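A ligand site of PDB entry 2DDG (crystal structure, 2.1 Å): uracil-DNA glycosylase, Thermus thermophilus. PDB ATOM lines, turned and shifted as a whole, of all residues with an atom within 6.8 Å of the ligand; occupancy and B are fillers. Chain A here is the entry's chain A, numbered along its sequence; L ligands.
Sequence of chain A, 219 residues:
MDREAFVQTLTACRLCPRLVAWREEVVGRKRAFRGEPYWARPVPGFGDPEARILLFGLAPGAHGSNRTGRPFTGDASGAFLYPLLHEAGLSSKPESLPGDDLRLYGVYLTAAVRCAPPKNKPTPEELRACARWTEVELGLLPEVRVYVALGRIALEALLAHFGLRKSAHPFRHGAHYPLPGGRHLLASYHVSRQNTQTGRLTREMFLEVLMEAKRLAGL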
ATOM      1  N   LEU A  10       2.249   7.301  15.998  1.00  0.00           N
ATOM      2  CA  LEU A  10       2.452   8.356  15.010  1.00  0.00           C
ATOM      3  C   LEU A  10       1.127   8.929  14.494  1.00  0.00           C
ATOM      4  O   LEU A  10       0.976  10.140  14.399  1.00  0.00           O
ATOM      5  CB  LEU A  10       3.257   7.846  13.811  1.00  0.00           C
ATOM      6  CG  LEU A  10       3.259   8.774  12.581  1.00  0.00           C
ATOM      7  CD1 LEU A  10       3.869  10.122  12.928  1.00  0.00           C
ATOM      8  CD2 LEU A  10       4.032   8.123  11.442  1.00  0.00           C
ATOM      9  N   THR A  11       0.193   8.053  14.155  1.00  0.00           N
ATOM     10  CA  THR A  11      -1.082   8.475  13.616  1.00  0.00           C
ATOM     11  C   THR A  11      -1.967   9.294  14.559  1.00  0.00           C
ATOM     12  O   THR A  11      -2.883   9.976  14.108  1.00  0.00           O
ATOM     13  CB  THR A  11      -1.883   7.267  13.060  1.00  0.00           C
ATOM     14  OG1 THR A  11      -2.006   6.268  14.075  1.00  0.00           O
ATOM     15  CG2 THR A  11      -1.149   6.669  11.857  1.00  0.00           C
ATOM     16  N   ALA A  12      -1.682   9.234  15.856  1.00  0.00           N
ATOM     17  CA  ALA A  12      -2.471   9.991  16.828  1.00  0.00           C
ATOM     18  C   ALA A  12      -1.747  11.278  17.229  1.00  0.00           C
ATOM     19  O   ALA A  12      -2.246  12.058  18.034  1.00  0.00           O
ATOM     20  CB  ALA A  12      -2.725   9.126  18.066  1.00  0.00           C
ATOM     21  N   CYS A  13      -0.571  11.501  16.647  1.00  0.00           N
ATOM     22  CA  CYS A  13       0.219  12.690  16.959  1.00  0.00           C
ATOM     23  C   CYS A  13      -0.468  13.995  16.551  1.00  0.00           C
ATOM     24  O   CYS A  13      -1.086  14.079  15.487  1.00  0.00           O
ATOM     25  CB  CYS A  13       1.568  12.589  16.274  1.00  0.00           C
ATOM     26  SG  CYS A  13       2.699  13.924  16.690  1.00  0.00           S
ATOM     27  N   ARG A  14      -0.356  15.013  17.401  1.00  0.00           N
ATOM     28  CA  ARG A  14      -0.967  16.322  17.146  1.00  0.00           C
ATOM     29  C   ARG A  14      -0.077  17.437  17.703  1.00  0.00           C
ATOM     30  O   ARG A  14      -0.577  18.456  18.170  1.00  0.00           O
ATOM     31  CB  ARG A  14      -2.346  16.401  17.809  1.00  0.00           C
ATOM     32  CG  ARG A  14      -3.316  15.293  17.429  1.00  0.00           C
ATOM     33  CD  ARG A  14      -4.589  15.360  18.272  1.00  0.00           C
ATOM     34  NE  ARG A  14      -5.400  16.541  17.971  1.00  0.00           N
ATOM     35  CZ  ARG A  14      -6.270  16.625  16.960  1.00  0.00           C
ATOM     36  NH1 ARG A  14      -6.442  15.588  16.144  1.00  0.00           N
ATOM     37  NH2 ARG A  14      -6.957  17.739  16.749  1.00  0.00           N
ATOM     38  N   LEU A  15       1.243  17.252  17.637  1.00  0.00           N
ATOM     39  CA  LEU A  15       2.179  18.240  18.169  1.00  0.00           C
ATOM     40  C   LEU A  15       2.251  19.566  17.428  1.00  0.00           C
ATOM     41  O   LEU A  15       2.610  20.592  18.024  1.00  0.00           O
ATOM     42  CB  LEU A  15       3.574  17.627  18.246  1.00  0.00           C
ATOM     43  CG  LEU A  15       3.721  16.446  19.205  1.00  0.00           C
ATOM     44  CD1 LEU A  15       5.135  15.867  19.108  1.00  0.00           C
ATOM     45  CD2 LEU A  15       3.424  16.909  20.624  1.00  0.00           C
ATOM     46  N   CYS A  16       1.920  19.566  16.143  1.00  0.00           N
ATOM     47  CA  CYS A  16       1.976  20.783  15.354  1.00  0.00           C
ATOM     48  C   CYS A  16       0.558  21.268  15.065  1.00  0.00           C
ATOM     49  O   CYS A  16      -0.132  20.754  14.180  1.00  0.00           O
ATOM     50  CB  CYS A  16       2.734  20.512  14.045  1.00  0.00           C
ATOM     51  SG  CYS A  16       4.418  19.876  14.299  1.00  0.00           S
ATOM     52  N   PRO A  17       0.095  22.271  15.837  1.00  0.00           N
ATOM     53  CA  PRO A  17      -1.250  22.796  15.643  1.00  0.00           C
ATOM     54  C   PRO A  17      -1.547  23.323  14.240  1.00  0.00           C
ATOM     55  O   PRO A  17      -2.640  23.100  13.723  1.00  0.00           O
ATOM     56  CB  PRO A  17      -1.375  23.862  16.739  1.00  0.00           C
ATOM     57  CG  PRO A  17       0.060  24.297  16.954  1.00  0.00           C
ATOM     58  CD  PRO A  17       0.804  22.990  16.908  1.00  0.00           C
ATOM     59  N   LEU A  19      -0.308  22.290  11.445  1.00  0.00           N
ATOM     60  CA  LEU A  19      -0.422  21.148  10.537  1.00  0.00           C
ATOM     61  C   LEU A  19      -1.644  20.271  10.836  1.00  0.00           C
ATOM     62  O   LEU A  19      -2.277  19.743   9.931  1.00  0.00           O
ATOM     63  CB  LEU A  19       0.866  20.325  10.579  1.00  0.00           C
ATOM     64  CG  LEU A  19       2.133  21.173  10.350  1.00  0.00           C
ATOM     65  CD1 LEU A  19       3.357  20.282  10.291  1.00  0.00           C
ATOM     66  CD2 LEU A  19       1.982  21.969   9.056  1.00  0.00           C
ATOM     67  N   VAL A  20      -1.984  20.127  12.107  1.00  0.00           N
ATOM     68  CA  VAL A  20      -3.155  19.337  12.488  1.00  0.00           C
ATOM     69  C   VAL A  20      -4.403  19.968  11.853  1.00  0.00           C
ATOM     70  O   VAL A  20      -5.360  19.273  11.488  1.00  0.00           O
ATOM     71  CB  VAL A  20      -3.328  19.306  14.023  1.00  0.00           C
ATOM     72  CG1 VAL A  20      -4.695  18.746  14.382  1.00  0.00           C
ATOM     73  CG2 VAL A  20      -2.228  18.455  14.654  1.00  0.00           C
ATOM     74  N   ARG A  23      -4.023  19.767   7.533  1.00  0.00           N
ATOM     75  CA  ARG A  23      -4.251  18.445   6.961  1.00  0.00           C
ATOM     76  C   ARG A  23      -5.736  18.121   6.789  1.00  0.00           C
ATOM     77  O   ARG A  23      -6.090  17.296   5.956  1.00  0.00           O
ATOM     78  CB  ARG A  23      -3.550  17.365   7.814  1.00  0.00           C
ATOM     79  CG  ARG A  23      -4.202  17.108   9.164  1.00  0.00           C
ATOM     80  CD  ARG A  23      -3.318  16.254  10.068  1.00  0.00           C
ATOM     81  NE  ARG A  23      -4.079  15.721  11.195  1.00  0.00           N
ATOM     82  CZ  ARG A  23      -3.537  15.218  12.296  1.00  0.00           C
ATOM     83  NH1 ARG A  23      -4.316  14.741  13.267  1.00  0.00           N
ATOM     84  NH2 ARG A  23      -2.221  15.192  12.447  1.00  0.00           N
ATOM     85  N   ARG A  41      -4.200  12.587   8.178  1.00  0.00           N
ATOM     86  CA  ARG A  41      -3.542  12.219   9.421  1.00  0.00           C
ATOM     87  C   ARG A  41      -2.049  12.083   9.147  1.00  0.00           C
ATOM     88  O   ARG A  41      -1.622  12.180   7.996  1.00  0.00           O
ATOM     89  CB  ARG A  41      -4.080  10.873   9.938  1.00  0.00           C
ATOM     90  CG  ARG A  41      -5.395  10.975  10.684  1.00  0.00           C
ATOM     91  CD  ARG A  41      -5.807   9.639  11.293  1.00  0.00           C
ATOM     92  NE  ARG A  41      -6.388   8.713  10.331  1.00  0.00           N
ATOM     93  CZ  ARG A  41      -7.481   8.972   9.618  1.00  0.00           C
ATOM     94  NH1 ARG A  41      -7.952   8.067   8.771  1.00  0.00           N
ATOM     95  NH2 ARG A  41      -8.091  10.138   9.745  1.00  0.00           N
ATOM     96  N   PRO A  42      -1.242  11.873  10.190  1.00  0.00           N
ATOM     97  CA  PRO A  42       0.197  11.722   9.967  1.00  0.00           C
ATOM     98  C   PRO A  42       0.403  10.565   8.995  1.00  0.00           C
ATOM     99  O   PRO A  42      -0.351   9.585   9.047  1.00  0.00           O
ATOM    100  CB  PRO A  42       0.738  11.416  11.360  1.00  0.00           C
ATOM    101  CG  PRO A  42      -0.219  12.189  12.265  1.00  0.00           C
ATOM    102  CD  PRO A  42      -1.561  11.870  11.640  1.00  0.00           C
ATOM    103  N   VAL A  43       1.380  10.663   8.107  1.00  0.00           N
ATOM    104  CA  VAL A  43       1.620   9.591   7.142  1.00  0.00           C
ATOM    105  C   VAL A  43       2.786   8.680   7.561  1.00  0.00           C
ATOM    106  O   VAL A  43       3.907   9.141   7.735  1.00  0.00           O
ATOM    107  CB  VAL A  43       1.888  10.176   5.725  1.00  0.00           C
ATOM    108  CG1 VAL A  43       2.325   9.058   4.759  1.00  0.00           C
ATOM    109  CG2 VAL A  43       0.628  10.862   5.211  1.00  0.00           C
ATOM    110  N   ALA A 112      10.628  14.139   5.985  1.00  0.00           N
ATOM    111  CA  ALA A 112      11.048  14.964   7.121  1.00  0.00           C
ATOM    112  C   ALA A 112       9.900  15.352   8.047  1.00  0.00           C
ATOM    113  O   ALA A 112      10.051  15.367   9.270  1.00  0.00           O
ATOM    114  CB  ALA A 112      11.757  16.212   6.610  1.00  0.00           C
ATOM    115  N   VAL A 113       8.767  15.718   7.449  1.00  0.00           N
ATOM    116  CA  VAL A 113       7.572  16.114   8.184  1.00  0.00           C
ATOM    117  C   VAL A 113       6.491  15.149   7.725  1.00  0.00           C
ATOM    118  O   VAL A 113       6.458  14.767   6.552  1.00  0.00           O
ATOM    119  CB  VAL A 113       7.204  17.574   7.888  1.00  0.00           C
ATOM    120  CG1 VAL A 113       5.783  17.856   8.280  1.00  0.00           C
ATOM    121  CG2 VAL A 113       8.151  18.490   8.645  1.00  0.00           C
ATOM    122  N   ARG A 114       5.593  14.759   8.626  1.00  0.00           N
ATOM    123  CA  ARG A 114       4.600  13.769   8.264  1.00  0.00           C
ATOM    124  C   ARG A 114       3.139  14.199   8.155  1.00  0.00           C
ATOM    125  O   ARG A 114       2.252  13.355   7.987  1.00  0.00           O
ATOM    126  CB  ARG A 114       4.757  12.581   9.207  1.00  0.00           C
ATOM    127  CG  ARG A 114       6.176  12.022   9.130  1.00  0.00           C
ATOM    128  CD  ARG A 114       6.523  11.003  10.222  1.00  0.00           C
ATOM    129  NE  ARG A 114       7.842  10.432   9.967  1.00  0.00           N
ATOM    130  CZ  ARG A 114       8.984  11.105  10.052  1.00  0.00           C
ATOM    131  NH1 ARG A 114       8.985  12.385  10.414  1.00  0.00           N
ATOM    132  NH2 ARG A 114      10.128  10.523   9.737  1.00  0.00           N
ATOM    133  N   CYS A 115       2.902  15.504   8.242  1.00  0.00           N
ATOM    134  CA  CYS A 115       1.555  16.073   8.116  1.00  0.00           C
ATOM    135  C   CYS A 115       1.639  17.192   7.082  1.00  0.00           C
ATOM    136  O   CYS A 115       2.593  17.979   7.075  1.00  0.00           O
ATOM    137  CB  CYS A 115       1.057  16.648   9.450  1.00  0.00           C
ATOM    138  SG  CYS A 115       0.569  15.414  10.673  1.00  0.00           S
ATOM    139  N   ALA A 116       0.639  17.246   6.206  1.00  0.00           N
ATOM    140  CA  ALA A 116       0.580  18.253   5.156  1.00  0.00           C
ATOM    141  C   ALA A 116       0.777  19.679   5.669  1.00  0.00           C
ATOM    142  O   ALA A 116       0.017  20.152   6.515  1.00  0.00           O
ATOM    143  CB  ALA A 116      -0.756  18.153   4.429  1.00  0.00           C
ATOM    144  N   GLU A 126       8.260  23.007  13.341  1.00  0.00           N
ATOM    145  CA  GLU A 126       7.522  21.807  12.966  1.00  0.00           C
ATOM    146  C   GLU A 126       8.524  20.723  12.554  1.00  0.00           C
ATOM    147  O   GLU A 126       8.313  19.533  12.799  1.00  0.00           O
ATOM    148  CB  GLU A 126       6.547  22.140  11.828  1.00  0.00           C
ATOM    149  CG  GLU A 126       5.559  23.227  12.234  1.00  0.00           C
ATOM    150  CD  GLU A 126       4.697  23.763  11.085  1.00  0.00           C
ATOM    151  OE1 GLU A 126       5.166  23.793   9.930  1.00  0.00           O
ATOM    152  OE2 GLU A 126       3.558  24.176  11.356  1.00  0.00           O
ATOM    153  N   ARG A 128      11.554  20.407  13.812  1.00  0.00           N
ATOM    154  CA  ARG A 128      12.142  19.929  15.060  1.00  0.00           C
ATOM    155  C   ARG A 128      11.234  18.940  15.767  1.00  0.00           C
ATOM    156  O   ARG A 128      11.702  17.954  16.352  1.00  0.00           O
ATOM    157  CB  ARG A 128      12.439  21.090  16.016  1.00  0.00           C
ATOM    158  CG  ARG A 128      13.612  21.972  15.591  1.00  0.00           C
ATOM    159  CD  ARG A 128      14.139  22.801  16.759  1.00  0.00           C
ATOM    160  NE  ARG A 128      13.176  23.806  17.221  1.00  0.00           N
ATOM    161  CZ  ARG A 128      12.977  24.978  16.634  1.00  0.00           C
ATOM    162  NH1 ARG A 128      13.679  25.311  15.552  1.00  0.00           N
ATOM    163  NH2 ARG A 128      12.078  25.819  17.115  1.00  0.00           N
ATOM    164  N   ALA A 129       9.933  19.189  15.710  1.00  0.00           N
ATOM    165  CA  ALA A 129       8.969  18.323  16.345  1.00  0.00           C
ATOM    166  C   ALA A 129       8.910  16.956  15.675  1.00  0.00           C
ATOM    167  O   ALA A 129       9.043  15.923  16.332  1.00  0.00           O
ATOM    168  CB  ALA A 129       7.590  18.979  16.324  1.00  0.00           C
ATOM    169  N   CYS A 130       8.736  16.935  14.362  1.00  0.00           N
ATOM    170  CA  CYS A 130       8.634  15.671  13.638  1.00  0.00           C
ATOM    171  C   CYS A 130       9.948  14.918  13.560  1.00  0.00           C
ATOM    172  O   CYS A 130       9.964  13.728  13.255  1.00  0.00           O
ATOM    173  CB  CYS A 130       8.072  15.894  12.233  1.00  0.00           C
ATOM    174  SG  CYS A 130       7.055  14.503  11.661  1.00  0.00           S
ATOM    175  N   ALA A 131      11.055  15.605  13.834  1.00  0.00           N
ATOM    176  CA  ALA A 131      12.377  14.976  13.791  1.00  0.00           C
ATOM    177  C   ALA A 131      12.424  13.832  14.809  1.00  0.00           C
ATOM    178  O   ALA A 131      13.235  12.907  14.673  1.00  0.00           O
ATOM    179  CB  ALA A 131      13.470  16.002  14.112  1.00  0.00           C
ATOM    180  N   ARG A 132      11.572  13.898  15.817  1.00  0.00           N
ATOM    181  CA  ARG A 132      11.523  12.841  16.832  1.00  0.00           C
ATOM    182  C   ARG A 132      10.998  11.564  16.195  1.00  0.00           C
ATOM    183  O   ARG A 132      11.397  10.457  16.573  1.00  0.00           O
ATOM    184  CB  ARG A 132      10.621  13.252  18.001  1.00  0.00           C
ATOM    185  CG  ARG A 132       9.132  13.287  17.677  1.00  0.00           C
ATOM    186  CD  ARG A 132       8.342  13.852  18.847  1.00  0.00           C
ATOM    187  NE  ARG A 132       8.745  15.226  19.146  1.00  0.00           N
ATOM    188  CZ  ARG A 132       8.390  15.896  20.244  1.00  0.00           C
ATOM    189  NH1 ARG A 132       7.621  15.314  21.155  1.00  0.00           N
ATOM    190  NH2 ARG A 132       8.810  17.144  20.422  1.00  0.00           N
ATOM    191  N   TRP A 133      10.099  11.701  15.229  1.00  0.00           N
ATOM    192  CA  TRP A 133       9.545  10.539  14.544  1.00  0.00           C
ATOM    193  C   TRP A 133      10.555   9.985  13.555  1.00  0.00           C
ATOM    194  O   TRP A 133      10.577   8.775  13.290  1.00  0.00           O
ATOM    195  CB  TRP A 133       8.238  10.915  13.825  1.00  0.00           C
ATOM    196  CG  TRP A 133       7.112  11.205  14.774  1.00  0.00           C
ATOM    197  CD1 TRP A 133       6.438  12.379  14.919  1.00  0.00           C
ATOM    198  CD2 TRP A 133       6.521  10.285  15.710  1.00  0.00           C
ATOM    199  NE1 TRP A 133       5.465  12.252  15.888  1.00  0.00           N
ATOM    200  CE2 TRP A 133       5.502  10.982  16.389  1.00  0.00           C
ATOM    201  CE3 TRP A 133       6.765   8.947  16.045  1.00  0.00           C
ATOM    202  CZ2 TRP A 133       4.714  10.383  17.375  1.00  0.00           C
ATOM    203  CZ3 TRP A 133       5.990   8.350  17.026  1.00  0.00           C
ATOM    204  CH2 TRP A 133       4.966   9.074  17.689  1.00  0.00           C
HETATM  205 FE1  LIG L   1       3.245  15.116  14.735  1.00  0.00          FE
HETATM  206 FE2  LIG L   1       5.003  15.255  12.727  1.00  0.00          FE
HETATM  207 FE3  LIG L   1       2.396  15.793  12.266  1.00  0.00          FE
HETATM  208 FE4  LIG L   1       3.902  17.508  13.722  1.00  0.00          FE
HETATM  209  S1  LIG L   1       4.159  16.988  11.538  1.00  0.00           S
HETATM  210  S2  LIG L   1       1.819  16.778  14.217  1.00  0.00           S
HETATM  211  S3  LIG L   1       5.277  16.079  14.804  1.00  0.00           S
HETATM  212  S4  LIG L   1       3.292  13.806  12.900  1.00  0.00           S
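The backbone NH of Cys 130 lies close to a sulfur (S3) of the ligand (3.6 Å). An iron atom (FE1) of the ligand is bound by the side-chain sulfur (SG) of Cys 13, 2.4 Å away. N of Cys 16 lies close to S2 of the ligand (3.4 Å). The side-chain sulfur (SG) of Cys 115 binds an iron atom (FE3) of the ligand (2.5 Å). SG of Cys 16 binds FE4 of the ligand. N of Leu 15 sits close to S2 of the ligand, at 3.5 Å. An iron atom (FE2) of the ligand is bound by the side-chain sulfur of Cys 130 (2.4 Å).
The guanidinium group of Arg 114 sits at hydrogen-bond distance from the backbone carbonyl oxygen of Ala 112, at 3.4 Å. The backbone carbonyl oxygen (O) of Cys 130 sits at hydrogen-bond distance from the guanidinium group (NH1) of Arg 114 (3.3 Å). The backbone carbonyl oxygen (O) of Cys 13 lies within hydrogen-bond range of the guanidinium group (NH2) of Arg 23, at 3.4 Å. SG of Cys 115 sits close to NH2 of Arg 23, at 3.3 Å. O of Arg 114 sits at hydrogen-bond distance from N of Val 43 (2.8 Å). The backbone carbonyl oxygen (O) of Ala 129 lies within hydrogen-bond range of the guanidinium group (NE) of Arg 132 (2.9 Å). The side-chain sulfur (SG) of Cys 13 sits close to the backbone NH (N) of Leu 15 (3.8 Å). SG of Cys 13 lies close to NE1 of Trp 133 (3.3 Å).
Merely in contact with the ligand: Leu 10 (3.7 Å), Leu 19 (3.6 Å), Pro 42 (3.8 Å), Val 113 (3.7 Å), Arg 114 (3.9 Å), Ala 129 (3.8 Å) and Trp 133 (3.8 Å). Hydrophobic or aromatic side chains within 4 Å of the ligand: Leu 10, Leu 19, Pro 42, Val 113 and Trp 133. Of the 26 residues printed, 12 come within 4 Å of the ligand.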
